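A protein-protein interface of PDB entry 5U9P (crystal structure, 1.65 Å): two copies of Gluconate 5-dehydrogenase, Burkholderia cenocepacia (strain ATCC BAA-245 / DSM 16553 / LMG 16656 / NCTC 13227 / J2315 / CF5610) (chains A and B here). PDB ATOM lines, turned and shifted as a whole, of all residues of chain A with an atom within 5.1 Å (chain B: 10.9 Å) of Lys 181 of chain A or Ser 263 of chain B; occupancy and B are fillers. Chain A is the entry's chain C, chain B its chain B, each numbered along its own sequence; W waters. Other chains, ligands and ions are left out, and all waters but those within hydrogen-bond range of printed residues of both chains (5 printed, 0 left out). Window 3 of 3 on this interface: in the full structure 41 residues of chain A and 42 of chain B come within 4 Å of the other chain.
The side-chain amide nitrogen of Gln 253 of chain A is in hydrogen-bond range of the side-chain hydroxyl of Thr 262 of chain B (3.2 Å). OG of Ser 263 of chain B lies within hydrogen-bond range of SG of Cys 184 of chain A (3.7 Å).
The side-chain carboxylate of Asp 258 of chain B is in hydrogen-bond range of the backbone NH of Gly 260 of chain B. The side-chain carboxylate of Asp 258 of chain B sits at hydrogen-bond distance from the backbone NH of Leu 261 of chain B. OD2 of Asp 258 of chain B sits at hydrogen-bond distance from OG1 of Thr 262 of chain B (2.8 Å). OG of Ser 263 of chain B lies within hydrogen-bond range of O of Gly 260 of chain B (2.8 Å). The side-chain sulfur (SG) of Cys 184 of chain A sits close to the side-chain amide oxygen (OD1) of Asn 251 of chain A (3.4 Å). The backbone carbonyl oxygen (O) of Asn 251 of chain A sits at hydrogen-bond distance from the side-chain amide nitrogen (NE2) of Gln 253 of chain A, at 3.1 Å.
Ser 263 of chain B touches Lys 181 of chain A (O to CB, 3.6 Å). SG of Cys 184 of chain A touches CB of Pro 225 of chain B, 3.8 Å away. Cys 184 of chain A touches Gly 260 of chain B. C of Gly 259 of chain B touches CB of Asn 251 of chain A (3.99 Å). Gly 260 of chain B touches Asn 251 of chain A. O of Gly 252 of chain A touches CB of Ser 263 of chain B, at 3.6 Å. Phe 256 of chain B touches Gln 253 of chain A (O to CG, 3.5 Å). OD1 of Asp 258 of chain B touches NE2 of Gln 253 of chain A (3.6 Å).
No residue of chain B comes within 4 Å of Met 178 of chain A. No residue of chain B comes within 4 Å of Thr 180 of chain A. Lys 181 of chain A touches just one residue of chain B: Ser 263 (3.6 Å). Cys 184 of chain A touches three residues of chain B. No residue of chain B comes within 4 Å of Ala 185 of chain A. Printed residues of chain B within 4 Å of Asn 251 of chain A: Gly 259 (3.99 Å) and Gly 260 (3.2 Å). Of chain B, only Phe 256 (3.5 Å), Asp 258 (3.6 Å) and Thr 262 (3.2 Å) come within 4 Å of Gln 253 of chain A. Printed residues of chain A within 4 Å of Pro 225 of chain B: Cys 184 (3.8 Å). Of the printed residues of chain A, Phe 256 of chain B touches Gln 253 (3.5 Å). Printed residues of chain A within 4 Å of Gly 259 of chain B: Asn 251 (3.99 Å). Printed residues of chain A within 4 Å of Gly 260 of chain B: Cys 184 and Asn 251. Of the printed residues of chain A, Ser 263 of chain B touches Lys 181 (3.6 Å), Cys 184 (3.7 Å) and Gly 252 (3.6 Å). The nearest residue of chain A that does not touch Ser 263 of chain B is Asn 251 of chain A (4.1 Å). The nearest printed residue of chain A that does not touch Pro 225 of chain B is Ala 185 of chain A (5.0 Å).
Of the 23 printed residues of chain B, 7 touch a printed residue of chain A. Hydrophobic or aromatic side chains of chain B that line the printed part of chain A: Pro 225 and Phe 256. Along chain B the printed residues that touch a printed residue of chain A span positions 225 to 263. Among the printed residues, no Asp or Glu carboxylate lies within 4 Å of a Lys or Arg side-chain nitrogen of the other chain.
1 position is printed for both chains. Of the 10 pairs that touch across the chains among the printed residues, none has its exchanged pair printed and touching as well.
Water W1 bridges OE1 of Gln 253 of chain A (2.5 Å) and OG1 of Thr 262 of chain B (3.3 Å). Water W5 lies within hydrogen-bond range of the side-chain hydroxyl (OG) of Ser 263 of chain B, the backbone carbonyl oxygen (O) of Lys 181 of chain A, the backbone NH (N) of Ala 185 of chain A and the side-chain sulfur (SG) of Cys 184 of chain A. Water W2 lies within hydrogen-bond range of OD1 of Asp 258 of chain B (2.7 Å), O of Phe 256 of chain B (2.8 Å) and N of Asn 251 of chain A (3.0 Å). Water W4 lies within hydrogen-bond range of the backbone NH (N) of Phe 256 of chain B (2.8 Å) and the side-chain amide oxygen (OE1) of Gln 253 of chain A (2.9 Å). Water W3 lies within hydrogen-bond range of the side-chain amino group of Lys 181 of chain A and the backbone carbonyl oxygen of Thr 262 of chain B.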
ATOM      1  N   ARG A 177      21.915  11.765  16.913  1.00  0.00           N
ATOM      2  CA  ARG A 177      23.162  11.627  16.171  1.00  0.00           C
ATOM      3  C   ARG A 177      22.905  11.103  14.762  1.00  0.00           C
ATOM      4  O   ARG A 177      23.477  11.611  13.790  1.00  0.00           O
ATOM      5  CB  ARG A 177      24.124  10.709  16.931  1.00  0.00           C
ATOM      6  CG  ARG A 177      25.515  10.627  16.306  1.00  0.00           C
ATOM      7  CD  ARG A 177      26.381   9.724  17.146  1.00  0.00           C
ATOM      8  NE  ARG A 177      27.735   9.652  16.621  1.00  0.00           N
ATOM      9  CZ  ARG A 177      28.676   8.925  17.201  1.00  0.00           C
ATOM     10  NH1 ARG A 177      28.365   8.237  18.297  1.00  0.00           N
ATOM     11  NH2 ARG A 177      29.903   8.866  16.680  1.00  0.00           N
ATOM     12  N   MET A 178      22.050  10.083  14.620  1.00  0.00           N
ATOM     13  CA  MET A 178      21.776   9.572  13.277  1.00  0.00           C
ATOM     14  C   MET A 178      20.876  10.526  12.493  1.00  0.00           C
ATOM     15  O   MET A 178      21.053  10.685  11.276  1.00  0.00           O
ATOM     16  CB  MET A 178      21.136   8.166  13.322  1.00  0.00           C
ATOM     17  CG  MET A 178      22.118   7.002  13.418  1.00  0.00           C
ATOM     18  SD  MET A 178      23.481   7.097  12.209  1.00  0.00           S
ATOM     19  CE  MET A 178      22.701   7.301  10.609  1.00  0.00           C
ATOM     20  N   LEU A 179      19.893  11.153  13.162  1.00  0.00           N
ATOM     21  CA  LEU A 179      19.052  12.119  12.463  1.00  0.00           C
ATOM     22  C   LEU A 179      19.891  13.239  11.874  1.00  0.00           C
ATOM     23  O   LEU A 179      19.597  13.727  10.778  1.00  0.00           O
ATOM     24  CB  LEU A 179      17.984  12.672  13.407  1.00  0.00           C
ATOM     25  CG  LEU A 179      16.889  13.541  12.770  1.00  0.00           C
ATOM     26  CD1 LEU A 179      16.006  12.769  11.782  1.00  0.00           C
ATOM     27  CD2 LEU A 179      16.041  14.192  13.868  1.00  0.00           C
ATOM     28  N   THR A 180      20.977  13.599  12.559  1.00  0.00           N
ATOM     29  CA  THR A 180      21.900  14.617  12.049  1.00  0.00           C
ATOM     30  C   THR A 180      22.519  14.172  10.729  1.00  0.00           C
ATOM     31  O   THR A 180      22.577  14.942   9.759  1.00  0.00           O
ATOM     32  CB  THR A 180      22.991  14.875  13.093  1.00  0.00           C
ATOM     33  OG1 THR A 180      22.398  15.399  14.282  1.00  0.00           O
ATOM     34  CG2 THR A 180      24.024  15.868  12.573  1.00  0.00           C
ATOM     35  N   LYS A 181      22.972  12.915  10.665  1.00  0.00           N
ATOM     36  CA  LYS A 181      23.501  12.413   9.396  1.00  0.00           C
ATOM     37  C   LYS A 181      22.417  12.410   8.326  1.00  0.00           C
ATOM     38  O   LYS A 181      22.683  12.701   7.155  1.00  0.00           O
ATOM     39  CB  LYS A 181      24.091  11.008   9.591  1.00  0.00           C
ATOM     40  CG  LYS A 181      25.138  10.951  10.686  1.00  0.00           C
ATOM     41  CD  LYS A 181      25.784   9.551  10.761  1.00  0.00           C
ATOM     42  CE  LYS A 181      26.545   9.332  12.077  1.00  0.00           C
ATOM     43  NZ  LYS A 181      27.277   8.019  12.048  1.00  0.00           N
ATOM     44  N   GLY A 182      21.179  12.124   8.721  1.00  0.00           N
ATOM     45  CA  GLY A 182      20.091  12.118   7.752  1.00  0.00           C
ATOM     46  C   GLY A 182      19.743  13.502   7.237  1.00  0.00           C
ATOM     47  O   GLY A 182      19.381  13.661   6.067  1.00  0.00           O
ATOM     48  N   MET A 183      19.815  14.517   8.103  1.00  0.00           N
ATOM     49  CA  MET A 183      19.644  15.896   7.648  1.00  0.00           C
ATOM     50  C   MET A 183      20.717  16.259   6.628  1.00  0.00           C
ATOM     51  O   MET A 183      20.429  16.885   5.602  1.00  0.00           O
ATOM     52  CB  MET A 183      19.697  16.860   8.843  1.00  0.00           C
ATOM     53  CG  MET A 183      18.548  16.716   9.864  1.00  0.00           C
ATOM     54  SD  MET A 183      18.830  17.937  11.169  1.00  0.00           S
ATOM     55  CE  MET A 183      17.585  17.417  12.350  1.00  0.00           C
ATOM     56  N   CYS A 184      21.966  15.857   6.884  1.00  0.00           N
ATOM     57  CA  CYS A 184      23.017  16.092   5.898  1.00  0.00           C
ATOM     58  C   CYS A 184      22.683  15.386   4.584  1.00  0.00           C
ATOM     59  O   CYS A 184      22.804  15.965   3.496  1.00  0.00           O
ATOM     60  CB  CYS A 184      24.359  15.610   6.477  1.00  0.00           C
ATOM     61  SG  CYS A 184      25.706  15.480   5.279  1.00  0.00           S
ATOM     62  N   ALA A 185      22.251  14.122   4.665  1.00  0.00           N
ATOM     63  CA  ALA A 185      22.004  13.367   3.440  1.00  0.00           C
ATOM     64  C   ALA A 185      20.929  14.034   2.588  1.00  0.00           C
ATOM     65  O   ALA A 185      21.047  14.080   1.358  1.00  0.00           O
ATOM     66  CB  ALA A 185      21.604  11.930   3.777  1.00  0.00           C
ATOM     67  N   ASN A 251      30.005  18.290   7.661  1.00  0.00           N
ATOM     68  CA  ASN A 251      28.586  17.981   7.502  1.00  0.00           C
ATOM     69  C   ASN A 251      28.330  16.575   8.017  1.00  0.00           C
ATOM     70  O   ASN A 251      29.151  15.672   7.817  1.00  0.00           O
ATOM     71  CB  ASN A 251      28.147  18.114   6.035  1.00  0.00           C
ATOM     72  CG  ASN A 251      26.732  18.708   5.893  1.00  0.00           C
ATOM     73  OD1 ASN A 251      25.902  18.548   6.792  1.00  0.00           O
ATOM     74  ND2 ASN A 251      26.448  19.358   4.751  1.00  0.00           N
ATOM     75  N   GLY A 252      27.202  16.407   8.711  1.00  0.00           N
ATOM     76  CA  GLY A 252      26.810  15.109   9.227  1.00  0.00           C
ATOM     77  C   GLY A 252      27.615  14.602  10.404  1.00  0.00           C
ATOM     78  O   GLY A 252      27.413  13.454  10.811  1.00  0.00           O
ATOM     79  N   GLN A 253      28.480  15.424  10.995  1.00  0.00           N
ATOM     80  CA  GLN A 253      29.388  14.980  12.052  1.00  0.00           C
ATOM     81  C   GLN A 253      28.841  15.327  13.425  1.00  0.00           C
ATOM     82  O   GLN A 253      28.103  16.298  13.585  1.00  0.00           O
ATOM     83  CB  GLN A 253      30.761  15.646  11.914  1.00  0.00           C
ATOM     84  CG  GLN A 253      31.380  15.481  10.551  1.00  0.00           C
ATOM     85  CD  GLN A 253      31.589  14.040  10.214  1.00  0.00           C
ATOM     86  OE1 GLN A 253      32.119  13.266  11.029  1.00  0.00           O
ATOM     87  NE2 GLN A 253      31.141  13.640   9.019  1.00  0.00           N
ATOM     88  N   VAL B 157      39.815  10.268   5.967  1.00  0.00           N
ATOM     89  CA  VAL B 157      38.616   9.420   5.887  1.00  0.00           C
ATOM     90  C   VAL B 157      38.993   7.974   6.145  1.00  0.00           C
ATOM     91  O   VAL B 157      38.211   7.203   6.725  1.00  0.00           O
ATOM     92  CB  VAL B 157      37.931   9.579   4.515  1.00  0.00           C
ATOM     93  CG1 VAL B 157      37.013   8.363   4.192  1.00  0.00           C
ATOM     94  CG2 VAL B 157      37.129  10.913   4.476  1.00  0.00           C
ATOM     95  N   GLU B 160      38.490   5.800   9.243  1.00  0.00           N
ATOM     96  CA  GLU B 160      37.185   5.175   9.487  1.00  0.00           C
ATOM     97  C   GLU B 160      36.732   4.250   8.366  1.00  0.00           C
ATOM     98  O   GLU B 160      36.205   3.164   8.644  1.00  0.00           O
ATOM     99  CB  GLU B 160      36.109   6.258   9.714  1.00  0.00           C
ATOM    100  CG  GLU B 160      34.693   5.668   9.896  1.00  0.00           C
ATOM    101  CD  GLU B 160      34.558   4.815  11.154  1.00  0.00           C
ATOM    102  OE1 GLU B 160      35.403   4.951  12.065  1.00  0.00           O
ATOM    103  OE2 GLU B 160      33.610   3.995  11.225  1.00  0.00           O
ATOM    104  N   LEU B 161      36.905   4.646   7.103  1.00  0.00           N
ATOM    105  CA  LEU B 161      36.336   3.912   5.979  1.00  0.00           C
ATOM    106  C   LEU B 161      37.433   3.542   4.993  1.00  0.00           C
ATOM    107  O   LEU B 161      38.234   4.394   4.601  1.00  0.00           O
ATOM    108  CB  LEU B 161      35.250   4.734   5.270  1.00  0.00           C
ATOM    109  CG  LEU B 161      34.011   5.078   6.092  1.00  0.00           C
ATOM    110  CD1 LEU B 161      33.042   5.888   5.221  1.00  0.00           C
ATOM    111  CD2 LEU B 161      33.284   3.833   6.628  1.00  0.00           C
ATOM    112  N   ARG B 177      44.539   7.780  14.641  1.00  0.00           N
ATOM    113  CA  ARG B 177      43.314   8.092  15.373  1.00  0.00           C
ATOM    114  C   ARG B 177      43.345   7.513  16.786  1.00  0.00           C
ATOM    115  O   ARG B 177      42.973   8.194  17.750  1.00  0.00           O
ATOM    116  CB  ARG B 177      42.092   7.586  14.604  1.00  0.00           C
ATOM    117  CG  ARG B 177      40.753   7.976  15.236  1.00  0.00           C
ATOM    118  CD  ARG B 177      39.652   7.396  14.400  1.00  0.00           C
ATOM    119  NE  ARG B 177      38.331   7.789  14.850  1.00  0.00           N
ATOM    120  CZ  ARG B 177      37.219   7.361  14.263  1.00  0.00           C
ATOM    121  NH1 ARG B 177      37.310   6.543  13.226  1.00  0.00           N
ATOM    122  NH2 ARG B 177      36.027   7.745  14.708  1.00  0.00           N
ATOM    123  N   ALA B 198      40.765  15.139  10.408  1.00  0.00           N
ATOM    124  CA  ALA B 198      40.675  14.184   9.310  1.00  0.00           C
ATOM    125  C   ALA B 198      40.099  14.847   8.070  1.00  0.00           C
ATOM    126  O   ALA B 198      38.870  14.941   7.940  1.00  0.00           O
ATOM    127  CB  ALA B 198      39.789  13.007   9.729  1.00  0.00           C
ATOM    128  N   GLY B 200      38.648  15.047   4.319  1.00  0.00           N
ATOM    129  CA  GLY B 200      38.118  14.188   3.278  1.00  0.00           C
ATOM    130  C   GLY B 200      38.969  14.267   2.024  1.00  0.00           C
ATOM    131  O   GLY B 200      40.196  14.159   2.100  1.00  0.00           O
ATOM    132  N   LYS B 222      29.329  12.218  -6.542  1.00  0.00           N
ATOM    133  CA  LYS B 222      28.110  11.523  -6.150  1.00  0.00           C
ATOM    134  C   LYS B 222      28.203  10.957  -4.738  1.00  0.00           C
ATOM    135  O   LYS B 222      27.180  10.833  -4.053  1.00  0.00           O
ATOM    136  CB  LYS B 222      27.822  10.397  -7.148  1.00  0.00           C
ATOM    137  CG  LYS B 222      27.319  10.893  -8.496  1.00  0.00           C
ATOM    138  CD  LYS B 222      27.320   9.785  -9.543  1.00  0.00           C
ATOM    139  CE  LYS B 222      26.976  10.351 -10.926  1.00  0.00           C
ATOM    140  NZ  LYS B 222      27.348   9.425 -12.047  1.00  0.00           N
ATOM    141  N   ARG B 223      29.407  10.577  -4.308  1.00  0.00           N
ATOM    142  CA  ARG B 223      29.592   9.937  -3.009  1.00  0.00           C
ATOM    143  C   ARG B 223      29.508  10.940  -1.862  1.00  0.00           C
ATOM    144  O   ARG B 223      29.088  10.572  -0.761  1.00  0.00           O
ATOM    145  CB  ARG B 223      30.944   9.209  -2.978  1.00  0.00           C
ATOM    146  CG  ARG B 223      31.278   8.542  -1.649  1.00  0.00           C
ATOM    147  CD  ARG B 223      30.316   7.415  -1.361  1.00  0.00           C
ATOM    148  NE  ARG B 223      30.621   6.753  -0.092  1.00  0.00           N
ATOM    149  CZ  ARG B 223      30.322   7.253   1.102  1.00  0.00           C
ATOM    150  NH1 ARG B 223      29.700   8.423   1.206  1.00  0.00           N
ATOM    151  NH2 ARG B 223      30.640   6.577   2.198  1.00  0.00           N
ATOM    152  N   THR B 224      29.890  12.195  -2.110  1.00  0.00           N
ATOM    153  CA  THR B 224      29.995  13.230  -1.078  1.00  0.00           C
ATOM    154  C   THR B 224      28.709  14.036  -1.027  1.00  0.00           C
ATOM    155  O   THR B 224      28.346  14.636  -2.050  1.00  0.00           O
ATOM    156  CB  THR B 224      31.160  14.169  -1.393  1.00  0.00           C
ATOM    157  OG1 THR B 224      32.333  13.405  -1.675  1.00  0.00           O
ATOM    158  CG2 THR B 224      31.431  15.135  -0.234  1.00  0.00           C
ATOM    159  N   PRO B 225      28.020  14.138   0.117  1.00  0.00           N
ATOM    160  CA  PRO B 225      26.799  14.966   0.144  1.00  0.00           C
ATOM    161  C   PRO B 225      27.020  16.386  -0.369  1.00  0.00           C
ATOM    162  O   PRO B 225      26.164  16.926  -1.085  1.00  0.00           O
ATOM    163  CB  PRO B 225      26.399  14.934   1.626  1.00  0.00           C
ATOM    164  CG  PRO B 225      26.848  13.540   2.085  1.00  0.00           C
ATOM    165  CD  PRO B 225      28.161  13.303   1.337  1.00  0.00           C
ATOM    166  N   ALA B 226      28.172  16.983  -0.049  1.00  0.00           N
ATOM    167  CA  ALA B 226      28.515  18.321  -0.528  1.00  0.00           C
ATOM    168  C   ALA B 226      28.709  18.378  -2.042  1.00  0.00           C
ATOM    169  O   ALA B 226      28.640  19.472  -2.624  1.00  0.00           O
ATOM    170  CB  ALA B 226      29.791  18.801   0.174  1.00  0.00           C
ATOM    171  N   GLY B 227      28.959  17.235  -2.683  1.00  0.00           N
ATOM    172  CA  GLY B 227      28.925  17.153  -4.131  1.00  0.00           C
ATOM    173  C   GLY B 227      30.163  17.655  -4.835  1.00  0.00           C
ATOM    174  O   GLY B 227      30.090  17.987  -6.028  1.00  0.00           O
ATOM    175  N   LEU B 255      38.064  15.091  14.307  1.00  0.00           N
ATOM    176  CA  LEU B 255      37.063  15.888  13.591  1.00  0.00           C
ATOM    177  C   LEU B 255      37.217  15.649  12.089  1.00  0.00           C
ATOM    178  O   LEU B 255      38.269  15.956  11.506  1.00  0.00           O
ATOM    179  CB  LEU B 255      37.239  17.373  13.923  1.00  0.00           C
ATOM    180  CG  LEU B 255      36.362  18.349  13.106  1.00  0.00           C
ATOM    181  CD1 LEU B 255      34.850  18.076  13.301  1.00  0.00           C
ATOM    182  CD2 LEU B 255      36.745  19.799  13.436  1.00  0.00           C
ATOM    183  N   PHE B 256      36.159  15.134  11.454  1.00  0.00           N
ATOM    184  CA  PHE B 256      36.186  14.876  10.019  1.00  0.00           C
ATOM    185  C   PHE B 256      35.646  16.081   9.256  1.00  0.00           C
ATOM    186  O   PHE B 256      34.537  16.558   9.524  1.00  0.00           O
ATOM    187  CB  PHE B 256      35.358  13.640   9.667  1.00  0.00           C
ATOM    188  CG  PHE B 256      35.971  12.352  10.145  1.00  0.00           C
ATOM    189  CD1 PHE B 256      36.625  11.501   9.251  1.00  0.00           C
ATOM    190  CD2 PHE B 256      35.924  12.000  11.477  1.00  0.00           C
ATOM    191  CE1 PHE B 256      37.203  10.308   9.686  1.00  0.00           C
ATOM    192  CE2 PHE B 256      36.512  10.820  11.916  1.00  0.00           C
ATOM    193  CZ  PHE B 256      37.143   9.964  11.010  1.00  0.00           C
ATOM    194  N   VAL B 257      36.430  16.547   8.293  1.00  0.00           N
ATOM    195  CA  VAL B 257      36.094  17.693   7.456  1.00  0.00           C
ATOM    196  C   VAL B 257      36.009  17.166   6.034  1.00  0.00           C
ATOM    197  O   VAL B 257      37.005  17.185   5.303  1.00  0.00           O
ATOM    198  CB  VAL B 257      37.152  18.804   7.581  1.00  0.00           C
ATOM    199  CG1 VAL B 257      36.711  20.018   6.737  1.00  0.00           C
ATOM    200  CG2 VAL B 257      37.338  19.210   9.054  1.00  0.00           C
ATOM    201  N   ASP B 258      34.837  16.622   5.650  1.00  0.00           N
ATOM    202  CA  ASP B 258      34.777  15.789   4.453  1.00  0.00           C
ATOM    203  C   ASP B 258      33.491  15.991   3.657  1.00  0.00           C
ATOM    204  O   ASP B 258      33.138  15.142   2.828  1.00  0.00           O
ATOM    205  CB  ASP B 258      34.927  14.286   4.825  1.00  0.00           C
ATOM    206  CG  ASP B 258      33.746  13.739   5.646  1.00  0.00           C
ATOM    207  OD1 ASP B 258      32.777  14.474   5.944  1.00  0.00           O
ATOM    208  OD2 ASP B 258      33.817  12.539   5.998  1.00  0.00           O
ATOM    209  N   GLY B 259      32.778  17.084   3.883  1.00  0.00           N
ATOM    210  CA  GLY B 259      31.610  17.326   3.073  1.00  0.00           C
ATOM    211  C   GLY B 259      30.493  16.350   3.331  1.00  0.00           C
ATOM    212  O   GLY B 259      29.577  16.260   2.522  1.00  0.00           O
ATOM    213  N   GLY B 260      30.550  15.612   4.440  1.00  0.00           N
ATOM    214  CA  GLY B 260      29.532  14.632   4.781  1.00  0.00           C
ATOM    215  C   GLY B 260      29.830  13.200   4.348  1.00  0.00           C
ATOM    216  O   GLY B 260      29.007  12.309   4.609  1.00  0.00           O
ATOM    217  N   LEU B 261      30.973  12.954   3.705  1.00  0.00           N
ATOM    218  CA  LEU B 261      31.254  11.628   3.135  1.00  0.00           C
ATOM    219  C   LEU B 261      31.077  10.507   4.164  1.00  0.00           C
ATOM    220  O   LEU B 261      30.369   9.519   3.907  1.00  0.00           O
ATOM    221  CB  LEU B 261      32.671  11.610   2.535  1.00  0.00           C
ATOM    222  CG  LEU B 261      32.979  10.432   1.584  1.00  0.00           C
ATOM    223  CD1 LEU B 261      34.064  10.858   0.567  1.00  0.00           C
ATOM    224  CD2 LEU B 261      33.385   9.146   2.318  1.00  0.00           C
ATOM    225  N   THR B 262      31.740  10.622   5.324  1.00  0.00           N
ATOM    226  CA  THR B 262      31.698   9.543   6.307  1.00  0.00           C
ATOM    227  C   THR B 262      30.337   9.396   6.977  1.00  0.00           C
ATOM    228  O   THR B 262      30.147   8.422   7.718  1.00  0.00           O
ATOM    229  CB  THR B 262      32.751   9.722   7.422  1.00  0.00           C
ATOM    230  OG1 THR B 262      32.644  11.030   8.010  1.00  0.00           O
ATOM    231  CG2 THR B 262      34.160   9.493   6.889  1.00  0.00           C
ATOM    232  N   SER B 263      29.398  10.323   6.746  1.00  0.00           N
ATOM    233  CA  SER B 263      28.108  10.230   7.418  1.00  0.00           C
ATOM    234  C   SER B 263      27.072   9.479   6.593  1.00  0.00           C
ATOM    235  O   SER B 263      25.985   9.187   7.106  1.00  0.00           O
ATOM    236  CB  SER B 263      27.567  11.637   7.753  1.00  0.00           C
ATOM    237  OG  SER B 263      27.076  12.334   6.606  1.00  0.00           O
ATOM    238  N   ALA B 264      27.387   9.146   5.343  1.00  0.00           N
ATOM    239  CA  ALA B 264      26.373   8.683   4.406  1.00  0.00           C
ATOM    240  C   ALA B 264      26.824   7.409   3.714  1.00  0.00           C
ATOM    241  O   ALA B 264      28.020   7.157   3.563  1.00  0.00           O
ATOM    242  CB  ALA B 264      26.091   9.753   3.327  1.00  0.00           C
ATOM    243  N   VAL B 265      25.853   6.619   3.264  1.00  0.00           N
ATOM    244  CA  VAL B 265      26.200   5.535   2.336  1.00  0.00           C
ATOM    245  C   VAL B 265      26.577   6.135   0.972  1.00  0.00           C
ATOM    246  O   VAL B 265      27.340   5.513   0.206  1.00  0.00           O
ATOM    247  CB  VAL B 265      25.066   4.498   2.168  1.00  0.00           C
ATOM    248  CG1 VAL B 265      24.693   3.871   3.499  1.00  0.00           C
ATOM    249  CG2 VAL B 265      23.856   5.112   1.477  1.00  0.00           C
ATOM    250  OXT VAL B 265      26.164   7.260   0.597  1.00  0.00           O
HETATM  251  O   HOH W   1      31.875  10.770  11.171  1.00  0.00           O
HETATM  252  O   HOH W   2      32.507  16.604   7.631  1.00  0.00           O
HETATM  253  O   HOH W   3      29.685   8.159  10.550  1.00  0.00           O
HETATM  254  O   HOH W   4      33.859  14.571  13.012  1.00  0.00           O
HETATM  255  O   HOH W   5      24.752  12.054   5.221  1.00  0.00           O
